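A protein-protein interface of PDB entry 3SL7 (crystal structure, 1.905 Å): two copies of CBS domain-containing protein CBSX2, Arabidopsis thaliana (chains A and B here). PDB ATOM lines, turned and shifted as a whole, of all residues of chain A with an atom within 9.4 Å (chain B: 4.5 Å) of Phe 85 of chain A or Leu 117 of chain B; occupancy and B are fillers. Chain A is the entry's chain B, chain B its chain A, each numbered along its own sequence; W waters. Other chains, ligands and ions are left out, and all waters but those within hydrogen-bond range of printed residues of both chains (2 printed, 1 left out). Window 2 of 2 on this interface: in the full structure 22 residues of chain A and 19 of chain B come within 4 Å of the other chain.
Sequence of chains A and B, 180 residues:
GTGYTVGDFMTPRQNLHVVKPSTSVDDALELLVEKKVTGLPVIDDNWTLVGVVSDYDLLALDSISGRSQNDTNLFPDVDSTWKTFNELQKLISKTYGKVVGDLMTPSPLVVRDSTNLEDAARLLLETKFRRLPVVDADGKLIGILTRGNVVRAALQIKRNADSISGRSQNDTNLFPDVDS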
ATOM      1  N   TRP A  82     -19.404  20.458  13.857  1.00  0.00           N
ATOM      2  CA  TRP A  82     -20.140  21.208  12.847  1.00  0.00           C
ATOM      3  C   TRP A  82     -19.192  22.026  11.979  1.00  0.00           C
ATOM      4  O   TRP A  82     -18.134  22.456  12.437  1.00  0.00           O
ATOM      5  CB  TRP A  82     -21.170  22.124  13.508  1.00  0.00           C
ATOM      6  CG  TRP A  82     -20.601  22.976  14.599  1.00  0.00           C
ATOM      7  CD1 TRP A  82     -20.344  22.598  15.885  1.00  0.00           C
ATOM      8  CD2 TRP A  82     -20.220  24.352  14.503  1.00  0.00           C
ATOM      9  NE1 TRP A  82     -19.827  23.653  16.594  1.00  0.00           N
ATOM     10  CE2 TRP A  82     -19.740  24.743  15.768  1.00  0.00           C
ATOM     11  CE3 TRP A  82     -20.237  25.294  13.469  1.00  0.00           C
ATOM     12  CZ2 TRP A  82     -19.283  26.031  16.027  1.00  0.00           C
ATOM     13  CZ3 TRP A  82     -19.783  26.572  13.729  1.00  0.00           C
ATOM     14  CH2 TRP A  82     -19.312  26.929  14.997  1.00  0.00           C
ATOM     15  N   LYS A  83     -19.577  22.240  10.726  1.00  0.00           N
ATOM     16  CA  LYS A  83     -18.746  22.993   9.795  1.00  0.00           C
ATOM     17  C   LYS A  83     -19.467  24.195   9.186  1.00  0.00           C
ATOM     18  O   LYS A  83     -18.839  25.053   8.562  1.00  0.00           O
ATOM     19  CB  LYS A  83     -18.209  22.070   8.702  1.00  0.00           C
ATOM     20  CG  LYS A  83     -17.232  21.025   9.224  1.00  0.00           C
ATOM     21  CD  LYS A  83     -17.708  19.617   8.918  1.00  0.00           C
ATOM     22  CE  LYS A  83     -17.786  19.370   7.415  1.00  0.00           C
ATOM     23  NZ  LYS A  83     -18.200  17.976   7.085  1.00  0.00           N
ATOM     24  N   THR A  84     -20.781  24.256   9.375  1.00  0.00           N
ATOM     25  CA  THR A  84     -21.556  25.413   8.947  1.00  0.00           C
ATOM     26  C   THR A  84     -22.562  25.770  10.023  1.00  0.00           C
ATOM     27  O   THR A  84     -22.889  24.938  10.870  1.00  0.00           O
ATOM     28  CB  THR A  84     -22.336  25.119   7.669  1.00  0.00           C
ATOM     29  OG1 THR A  84     -23.388  24.198   7.968  1.00  0.00           O
ATOM     30  CG2 THR A  84     -21.416  24.521   6.614  1.00  0.00           C
ATOM     31  N   PHE A  85     -23.070  26.998   9.974  1.00  0.00           N
ATOM     32  CA  PHE A  85     -24.068  27.419  10.940  1.00  0.00           C
ATOM     33  C   PHE A  85     -25.326  26.558  10.834  1.00  0.00           C
ATOM     34  O   PHE A  85     -25.933  26.202  11.845  1.00  0.00           O
ATOM     35  CB  PHE A  85     -24.418  28.894  10.778  1.00  0.00           C
ATOM     36  CG  PHE A  85     -25.215  29.438  11.917  1.00  0.00           C
ATOM     37  CD1 PHE A  85     -24.607  29.673  13.143  1.00  0.00           C
ATOM     38  CD2 PHE A  85     -26.568  29.694  11.778  1.00  0.00           C
ATOM     39  CE1 PHE A  85     -25.332  30.164  14.207  1.00  0.00           C
ATOM     40  CE2 PHE A  85     -27.301  30.190  12.836  1.00  0.00           C
ATOM     41  CZ  PHE A  85     -26.677  30.424  14.059  1.00  0.00           C
ATOM     42  N   ASN A  86     -25.714  26.222   9.613  1.00  0.00           N
ATOM     43  CA  ASN A  86     -26.877  25.369   9.418  1.00  0.00           C
ATOM     44  C   ASN A  86     -26.715  23.999  10.098  1.00  0.00           C
ATOM     45  O   ASN A  86     -27.640  23.504  10.753  1.00  0.00           O
ATOM     46  CB  ASN A  86     -27.193  25.210   7.930  1.00  0.00           C
ATOM     47  CG  ASN A  86     -28.563  24.612   7.691  1.00  0.00           C
ATOM     48  OD1 ASN A  86     -29.577  25.307   7.772  1.00  0.00           O
ATOM     49  ND2 ASN A  86     -28.602  23.318   7.396  1.00  0.00           N
ATOM     50  N   GLU A  87     -25.545  23.384   9.944  1.00  0.00           N
ATOM     51  CA  GLU A  87     -25.277  22.096  10.587  1.00  0.00           C
ATOM     52  C   GLU A  87     -25.329  22.239  12.102  1.00  0.00           C
ATOM     53  O   GLU A  87     -25.841  21.373  12.805  1.00  0.00           O
ATOM     54  CB  GLU A  87     -23.899  21.573  10.195  1.00  0.00           C
ATOM     55  CG  GLU A  87     -23.743  21.215   8.728  1.00  0.00           C
ATOM     56  CD  GLU A  87     -22.352  20.691   8.414  1.00  0.00           C
ATOM     57  OE1 GLU A  87     -21.473  20.744   9.306  1.00  0.00           O
ATOM     58  OE2 GLU A  87     -22.138  20.221   7.277  1.00  0.00           O
ATOM     59  N   LEU A  88     -24.776  23.341  12.599  1.00  0.00           N
ATOM     60  CA  LEU A  88     -24.803  23.644  14.019  1.00  0.00           C
ATOM     61  C   LEU A  88     -26.234  23.772  14.538  1.00  0.00           C
ATOM     62  O   LEU A  88     -26.568  23.224  15.589  1.00  0.00           O
ATOM     63  CB  LEU A  88     -24.040  24.938  14.293  1.00  0.00           C
ATOM     64  CG  LEU A  88     -24.103  25.404  15.743  1.00  0.00           C
ATOM     65  CD1 LEU A  88     -23.506  24.330  16.649  1.00  0.00           C
ATOM     66  CD2 LEU A  88     -23.366  26.709  15.888  1.00  0.00           C
ATOM     67  N   GLN A  89     -27.078  24.498  13.806  1.00  0.00           N
ATOM     68  CA  GLN A  89     -28.474  24.630  14.198  1.00  0.00           C
ATOM     69  C   GLN A  89     -29.150  23.272  14.239  1.00  0.00           C
ATOM     70  O   GLN A  89     -29.980  23.020  15.106  1.00  0.00           O
ATOM     71  CB  GLN A  89     -29.233  25.580  13.255  1.00  0.00           C
ATOM     72  CG  GLN A  89     -28.797  27.028  13.401  1.00  0.00           C
ATOM     73  CD  GLN A  89     -29.739  27.990  12.703  1.00  0.00           C
ATOM     74  OE1 GLN A  89     -29.692  28.135  11.488  1.00  0.00           O
ATOM     75  NE2 GLN A  89     -30.597  28.651  13.474  1.00  0.00           N
ATOM     76  N   LYS A  90     -28.802  22.406  13.293  1.00  0.00           N
ATOM     77  CA  LYS A  90     -29.386  21.069  13.260  1.00  0.00           C
ATOM     78  C   LYS A  90     -29.019  20.341  14.541  1.00  0.00           C
ATOM     79  O   LYS A  90     -29.855  19.707  15.175  1.00  0.00           O
ATOM     80  CB  LYS A  90     -28.896  20.279  12.043  1.00  0.00           C
ATOM     81  CG  LYS A  90     -29.521  20.698  10.717  1.00  0.00           C
ATOM     82  CD  LYS A  90     -29.334  19.612   9.660  1.00  0.00           C
ATOM     83  CE  LYS A  90     -29.935  20.015   8.317  1.00  0.00           C
ATOM     84  NZ  LYS A  90     -28.956  20.734   7.457  1.00  0.00           N
ATOM     85  N   LEU A  91     -27.755  20.452  14.937  1.00  0.00           N
ATOM     86  CA  LEU A  91     -27.289  19.818  16.168  1.00  0.00           C
ATOM     87  C   LEU A  91     -27.996  20.407  17.380  1.00  0.00           C
ATOM     88  O   LEU A  91     -28.502  19.679  18.229  1.00  0.00           O
ATOM     89  CB  LEU A  91     -25.773  19.987  16.330  1.00  0.00           C
ATOM     90  CG  LEU A  91     -24.901  19.247  15.311  1.00  0.00           C
ATOM     91  CD1 LEU A  91     -23.434  19.555  15.529  1.00  0.00           C
ATOM     92  CD2 LEU A  91     -25.151  17.751  15.391  1.00  0.00           C
ATOM     93  N   ILE A  92     -28.020  21.732  17.462  1.00  0.00           N
ATOM     94  CA  ILE A  92     -28.700  22.396  18.567  1.00  0.00           C
ATOM     95  C   ILE A  92     -30.174  21.972  18.661  1.00  0.00           C
ATOM     96  O   ILE A  92     -30.717  21.839  19.754  1.00  0.00           O
ATOM     97  CB  ILE A  92     -28.615  23.926  18.449  1.00  0.00           C
ATOM     98  CG1 ILE A  92     -27.168  24.378  18.592  1.00  0.00           C
ATOM     99  CG2 ILE A  92     -29.482  24.591  19.523  1.00  0.00           C
ATOM    100  CD1 ILE A  92     -26.616  24.101  19.943  1.00  0.00           C
ATOM    101  N   SER A  93     -30.814  21.750  17.519  1.00  0.00           N
ATOM    102  CA  SER A  93     -32.234  21.400  17.522  1.00  0.00           C
ATOM    103  C   SER A  93     -32.457  20.023  18.139  1.00  0.00           C
ATOM    104  O   SER A  93     -33.497  19.766  18.746  1.00  0.00           O
ATOM    105  CB  SER A  93     -32.825  21.459  16.110  1.00  0.00           C
ATOM    106  OG  SER A  93     -32.449  20.327  15.342  1.00  0.00           O
ATOM    107  N   TYR B   4     -28.892  37.106  10.770  1.00  0.00           N
ATOM    108  CA  TYR B   4     -28.065  37.719  11.804  1.00  0.00           C
ATOM    109  C   TYR B   4     -26.679  38.127  11.290  1.00  0.00           C
ATOM    110  O   TYR B   4     -26.229  37.672  10.241  1.00  0.00           O
ATOM    111  CB  TYR B   4     -27.938  36.799  13.016  1.00  0.00           C
ATOM    112  CG  TYR B   4     -29.229  36.632  13.785  1.00  0.00           C
ATOM    113  CD1 TYR B   4     -30.116  35.608  13.478  1.00  0.00           C
ATOM    114  CD2 TYR B   4     -29.558  37.496  14.820  1.00  0.00           C
ATOM    115  CE1 TYR B   4     -31.295  35.450  14.178  1.00  0.00           C
ATOM    116  CE2 TYR B   4     -30.736  37.345  15.529  1.00  0.00           C
ATOM    117  CZ  TYR B   4     -31.598  36.322  15.201  1.00  0.00           C
ATOM    118  OH  TYR B   4     -32.769  36.167  15.902  1.00  0.00           O
ATOM    119  N   THR B   5     -26.017  39.007  12.029  1.00  0.00           N
ATOM    120  CA  THR B   5     -24.707  39.481  11.631  1.00  0.00           C
ATOM    121  C   THR B   5     -23.695  39.236  12.761  1.00  0.00           C
ATOM    122  O   THR B   5     -24.069  38.989  13.909  1.00  0.00           O
ATOM    123  CB  THR B   5     -24.743  40.979  11.324  1.00  0.00           C
ATOM    124  OG1 THR B   5     -25.077  41.687  12.520  1.00  0.00           O
ATOM    125  CG2 THR B   5     -25.800  41.310  10.225  1.00  0.00           C
ATOM    126  N   VAL B   6     -22.414  39.315  12.432  1.00  0.00           N
ATOM    127  CA  VAL B   6     -21.369  39.167  13.437  1.00  0.00           C
ATOM    128  C   VAL B   6     -21.634  40.081  14.634  1.00  0.00           C
ATOM    129  O   VAL B   6     -21.515  39.664  15.782  1.00  0.00           O
ATOM    130  CB  VAL B   6     -19.989  39.461  12.833  1.00  0.00           C
ATOM    131  CG1 VAL B   6     -18.917  39.580  13.929  1.00  0.00           C
ATOM    132  CG2 VAL B   6     -19.633  38.385  11.827  1.00  0.00           C
ATOM    133  N   PHE B   9     -23.518  38.921  17.779  1.00  0.00           N
ATOM    134  CA  PHE B   9     -23.054  37.841  18.663  1.00  0.00           C
ATOM    135  C   PHE B   9     -21.565  37.818  18.977  1.00  0.00           C
ATOM    136  O   PHE B   9     -21.099  36.941  19.697  1.00  0.00           O
ATOM    137  CB  PHE B   9     -23.464  36.493  18.091  1.00  0.00           C
ATOM    138  CG  PHE B   9     -24.949  36.318  17.989  1.00  0.00           C
ATOM    139  CD1 PHE B   9     -25.689  35.922  19.088  1.00  0.00           C
ATOM    140  CD2 PHE B   9     -25.602  36.557  16.796  1.00  0.00           C
ATOM    141  CE1 PHE B   9     -27.048  35.762  18.999  1.00  0.00           C
ATOM    142  CE2 PHE B   9     -26.968  36.397  16.701  1.00  0.00           C
ATOM    143  CZ  PHE B   9     -27.693  36.002  17.806  1.00  0.00           C
ATOM    144  N   THR B 115     -20.987  41.762   8.893  1.00  0.00           N
ATOM    145  CA  THR B 115     -20.796  40.505   8.184  1.00  0.00           C
ATOM    146  C   THR B 115     -21.888  39.520   8.553  1.00  0.00           C
ATOM    147  O   THR B 115     -22.232  39.374   9.719  1.00  0.00           O
ATOM    148  CB  THR B 115     -19.414  39.898   8.493  1.00  0.00           C
ATOM    149  OG1 THR B 115     -18.402  40.794   8.031  1.00  0.00           O
ATOM    150  CG2 THR B 115     -19.238  38.565   7.793  1.00  0.00           C
ATOM    151  N   ASN B 116     -22.443  38.867   7.538  1.00  0.00           N
ATOM    152  CA  ASN B 116     -23.464  37.848   7.728  1.00  0.00           C
ATOM    153  C   ASN B 116     -22.936  36.738   8.630  1.00  0.00           C
ATOM    154  O   ASN B 116     -21.827  36.249   8.443  1.00  0.00           O
ATOM    155  CB  ASN B 116     -23.904  37.293   6.371  1.00  0.00           C
ATOM    156  CG  ASN B 116     -24.765  36.051   6.498  1.00  0.00           C
ATOM    157  OD1 ASN B 116     -24.270  34.924   6.427  1.00  0.00           O
ATOM    158  ND2 ASN B 116     -26.063  36.253   6.683  1.00  0.00           N
ATOM    159  N   LEU B 117     -23.727  36.360   9.627  1.00  0.00           N
ATOM    160  CA  LEU B 117     -23.273  35.401  10.634  1.00  0.00           C
ATOM    161  C   LEU B 117     -22.896  34.057  10.027  1.00  0.00           C
ATOM    162  O   LEU B 117     -21.879  33.473  10.405  1.00  0.00           O
ATOM    163  CB  LEU B 117     -24.322  35.204  11.726  1.00  0.00           C
ATOM    164  CG  LEU B 117     -23.890  34.305  12.890  1.00  0.00           C
ATOM    165  CD1 LEU B 117     -22.736  34.942  13.638  1.00  0.00           C
ATOM    166  CD2 LEU B 117     -25.049  34.048  13.823  1.00  0.00           C
ATOM    167  N   GLU B 118     -23.712  33.556   9.104  1.00  0.00           N
ATOM    168  CA  GLU B 118     -23.430  32.270   8.461  1.00  0.00           C
ATOM    169  C   GLU B 118     -22.135  32.307   7.657  1.00  0.00           C
ATOM    170  O   GLU B 118     -21.385  31.343   7.656  1.00  0.00           O
ATOM    171  CB  GLU B 118     -24.596  31.820   7.570  1.00  0.00           C
ATOM    172  CG  GLU B 118     -25.914  31.727   8.327  1.00  0.00           C
ATOM    173  CD  GLU B 118     -26.943  30.815   7.657  1.00  0.00           C
ATOM    174  OE1 GLU B 118     -26.543  29.940   6.857  1.00  0.00           O
ATOM    175  OE2 GLU B 118     -28.152  30.971   7.938  1.00  0.00           O
ATOM    176  N   ASP B 119     -21.885  33.409   6.955  1.00  0.00           N
ATOM    177  CA  ASP B 119     -20.618  33.574   6.250  1.00  0.00           C
ATOM    178  C   ASP B 119     -19.464  33.560   7.250  1.00  0.00           C
ATOM    179  O   ASP B 119     -18.478  32.858   7.056  1.00  0.00           O
ATOM    180  CB  ASP B 119     -20.600  34.885   5.469  1.00  0.00           C
ATOM    181  CG  ASP B 119     -21.367  34.797   4.167  1.00  0.00           C
ATOM    182  OD1 ASP B 119     -22.027  33.765   3.931  1.00  0.00           O
ATOM    183  OD2 ASP B 119     -21.311  35.764   3.377  1.00  0.00           O
ATOM    184  N   ALA B 120     -19.595  34.341   8.318  1.00  0.00           N
ATOM    185  CA  ALA B 120     -18.542  34.417   9.318  1.00  0.00           C
ATOM    186  C   ALA B 120     -18.299  33.055   9.957  1.00  0.00           C
ATOM    187  O   ALA B 120     -17.163  32.659  10.186  1.00  0.00           O
ATOM    188  CB  ALA B 120     -18.879  35.461  10.370  1.00  0.00           C
ATOM    189  N   ALA B 121     -19.371  32.321  10.221  1.00  0.00           N
ATOM    190  CA  ALA B 121     -19.244  31.013  10.843  1.00  0.00           C
ATOM    191  C   ALA B 121     -18.377  30.082   9.990  1.00  0.00           C
ATOM    192  O   ALA B 121     -17.512  29.372  10.500  1.00  0.00           O
ATOM    193  CB  ALA B 121     -20.623  30.411  11.080  1.00  0.00           C
ATOM    194  N   VAL B 150     -20.541  31.671  18.193  1.00  0.00           N
ATOM    195  CA  VAL B 150     -21.416  31.148  17.150  1.00  0.00           C
ATOM    196  C   VAL B 150     -22.376  30.132  17.746  1.00  0.00           C
ATOM    197  O   VAL B 150     -23.555  30.111  17.418  1.00  0.00           O
ATOM    198  CB  VAL B 150     -20.615  30.524  15.986  1.00  0.00           C
ATOM    199  CG1 VAL B 150     -21.556  29.875  14.976  1.00  0.00           C
ATOM    200  CG2 VAL B 150     -19.742  31.584  15.311  1.00  0.00           C
ATOM    201  N   ALA B 153     -25.035  31.906  19.502  1.00  0.00           N
ATOM    202  CA  ALA B 153     -26.027  32.436  18.564  1.00  0.00           C
ATOM    203  C   ALA B 153     -27.051  31.380  18.175  1.00  0.00           C
ATOM    204  O   ALA B 153     -28.252  31.636  18.201  1.00  0.00           O
ATOM    205  CB  ALA B 153     -25.357  33.016  17.323  1.00  0.00           C
ATOM    206  N   ALA B 154     -26.580  30.189  17.815  1.00  0.00           N
ATOM    207  CA  ALA B 154     -27.493  29.096  17.468  1.00  0.00           C
ATOM    208  C   ALA B 154     -28.442  28.777  18.624  1.00  0.00           C
ATOM    209  O   ALA B 154     -29.630  28.527  18.420  1.00  0.00           O
ATOM    210  CB  ALA B 154     -26.711  27.855  17.061  1.00  0.00           C
ATOM    211  N   ILE B 157     -31.031  31.634  19.088  1.00  0.00           N
ATOM    212  CA  ILE B 157     -31.977  31.580  17.991  1.00  0.00           C
ATOM    213  C   ILE B 157     -33.025  30.506  18.246  1.00  0.00           C
ATOM    214  O   ILE B 157     -34.221  30.752  18.112  1.00  0.00           O
ATOM    215  CB  ILE B 157     -31.254  31.341  16.656  1.00  0.00           C
ATOM    216  CG1 ILE B 157     -30.381  32.550  16.318  1.00  0.00           C
ATOM    217  CG2 ILE B 157     -32.249  31.089  15.545  1.00  0.00           C
ATOM    218  CD1 ILE B 157     -29.501  32.345  15.097  1.00  0.00           C
HETATM  219  O   HOH W   1     -25.122  27.760   7.441  1.00  0.00           O
HETATM  220  O   HOH W   2     -22.263  28.886   8.028  1.00  0.00           O
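N of Leu 117 of chain B sits at hydrogen-bond distance from O of Tyr 4 of chain B.
Trp 82 of chain A touches Val 150 of chain B.
Phe 85 of chain A touches Leu 117 of chain B.
Phe 85 of chain A touches Val 150 of chain B (CD1 to CG1, 3.6 Å).
Phe 85 of chain A touches Ala 154 of chain B (CZ to CA, 3.7 Å).
Ile 157 of chain B touches Phe 85 of chain A (CD1 to CZ, 3.6 Å).
Leu 88 of chain A touches Val 150 of chain B.
CB of Ala 154 of chain B touches CD2 of Leu 88 of chain A, at 3.7 Å.
Ile 157 of chain B touches Gln 89 of chain A.
Ile 92 of chain A touches Ala 154 of chain B (CG1 to CB, 3.8 Å).
Of the printed residues of chain B, Trp 82 of chain A touches Val 150.
Printed residues of chain B within 4 Å of Phe 85 of chain A: Leu 117, Val 150, Ala 154 and Ile 157.
Printed residues of chain B within 4 Å of Leu 88 of chain A: Val 150 (3.7 Å) and Ala 154 (3.7 Å).
Printed residues of chain B within 4 Å of Gln 89 of chain A: Ile 157.
No residue of chain A comes within 4 Å of Asn 116 of chain B.
Of chain A, only Phe 85 comes within 4 Å of Leu 117 of chain B.
No residue of chain A comes within 4 Å of Ala 120 of chain B.
Of the printed residues of chain A, Ile 157 of chain B touches Phe 85 (3.6 Å) and Gln 89 (3.6 Å).
The nearest printed residue of chain B that does not touch Trp 82 of chain A is Ala 121 of chain B (4.7 Å).
Hydrophobic or aromatic side chains of chain A that line the printed part of chain B: Trp 82, Phe 85, Leu 88 and Ile 92.
No position is printed for both chains.
Water W2 bridges the backbone carbonyl oxygen of Glu 118 of chain B (2.6 Å) and the backbone NH of Phe 85 of chain A (2.8 Å).
Water W1 lies within hydrogen-bond range of the side-chain carboxylate (OE1) of Glu 118 of chain B (2.7 Å), the backbone NH (N) of Asn 86 of chain A (2.7 Å) and the backbone NH (N) of Phe 85 of chain A (3.3 Å).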
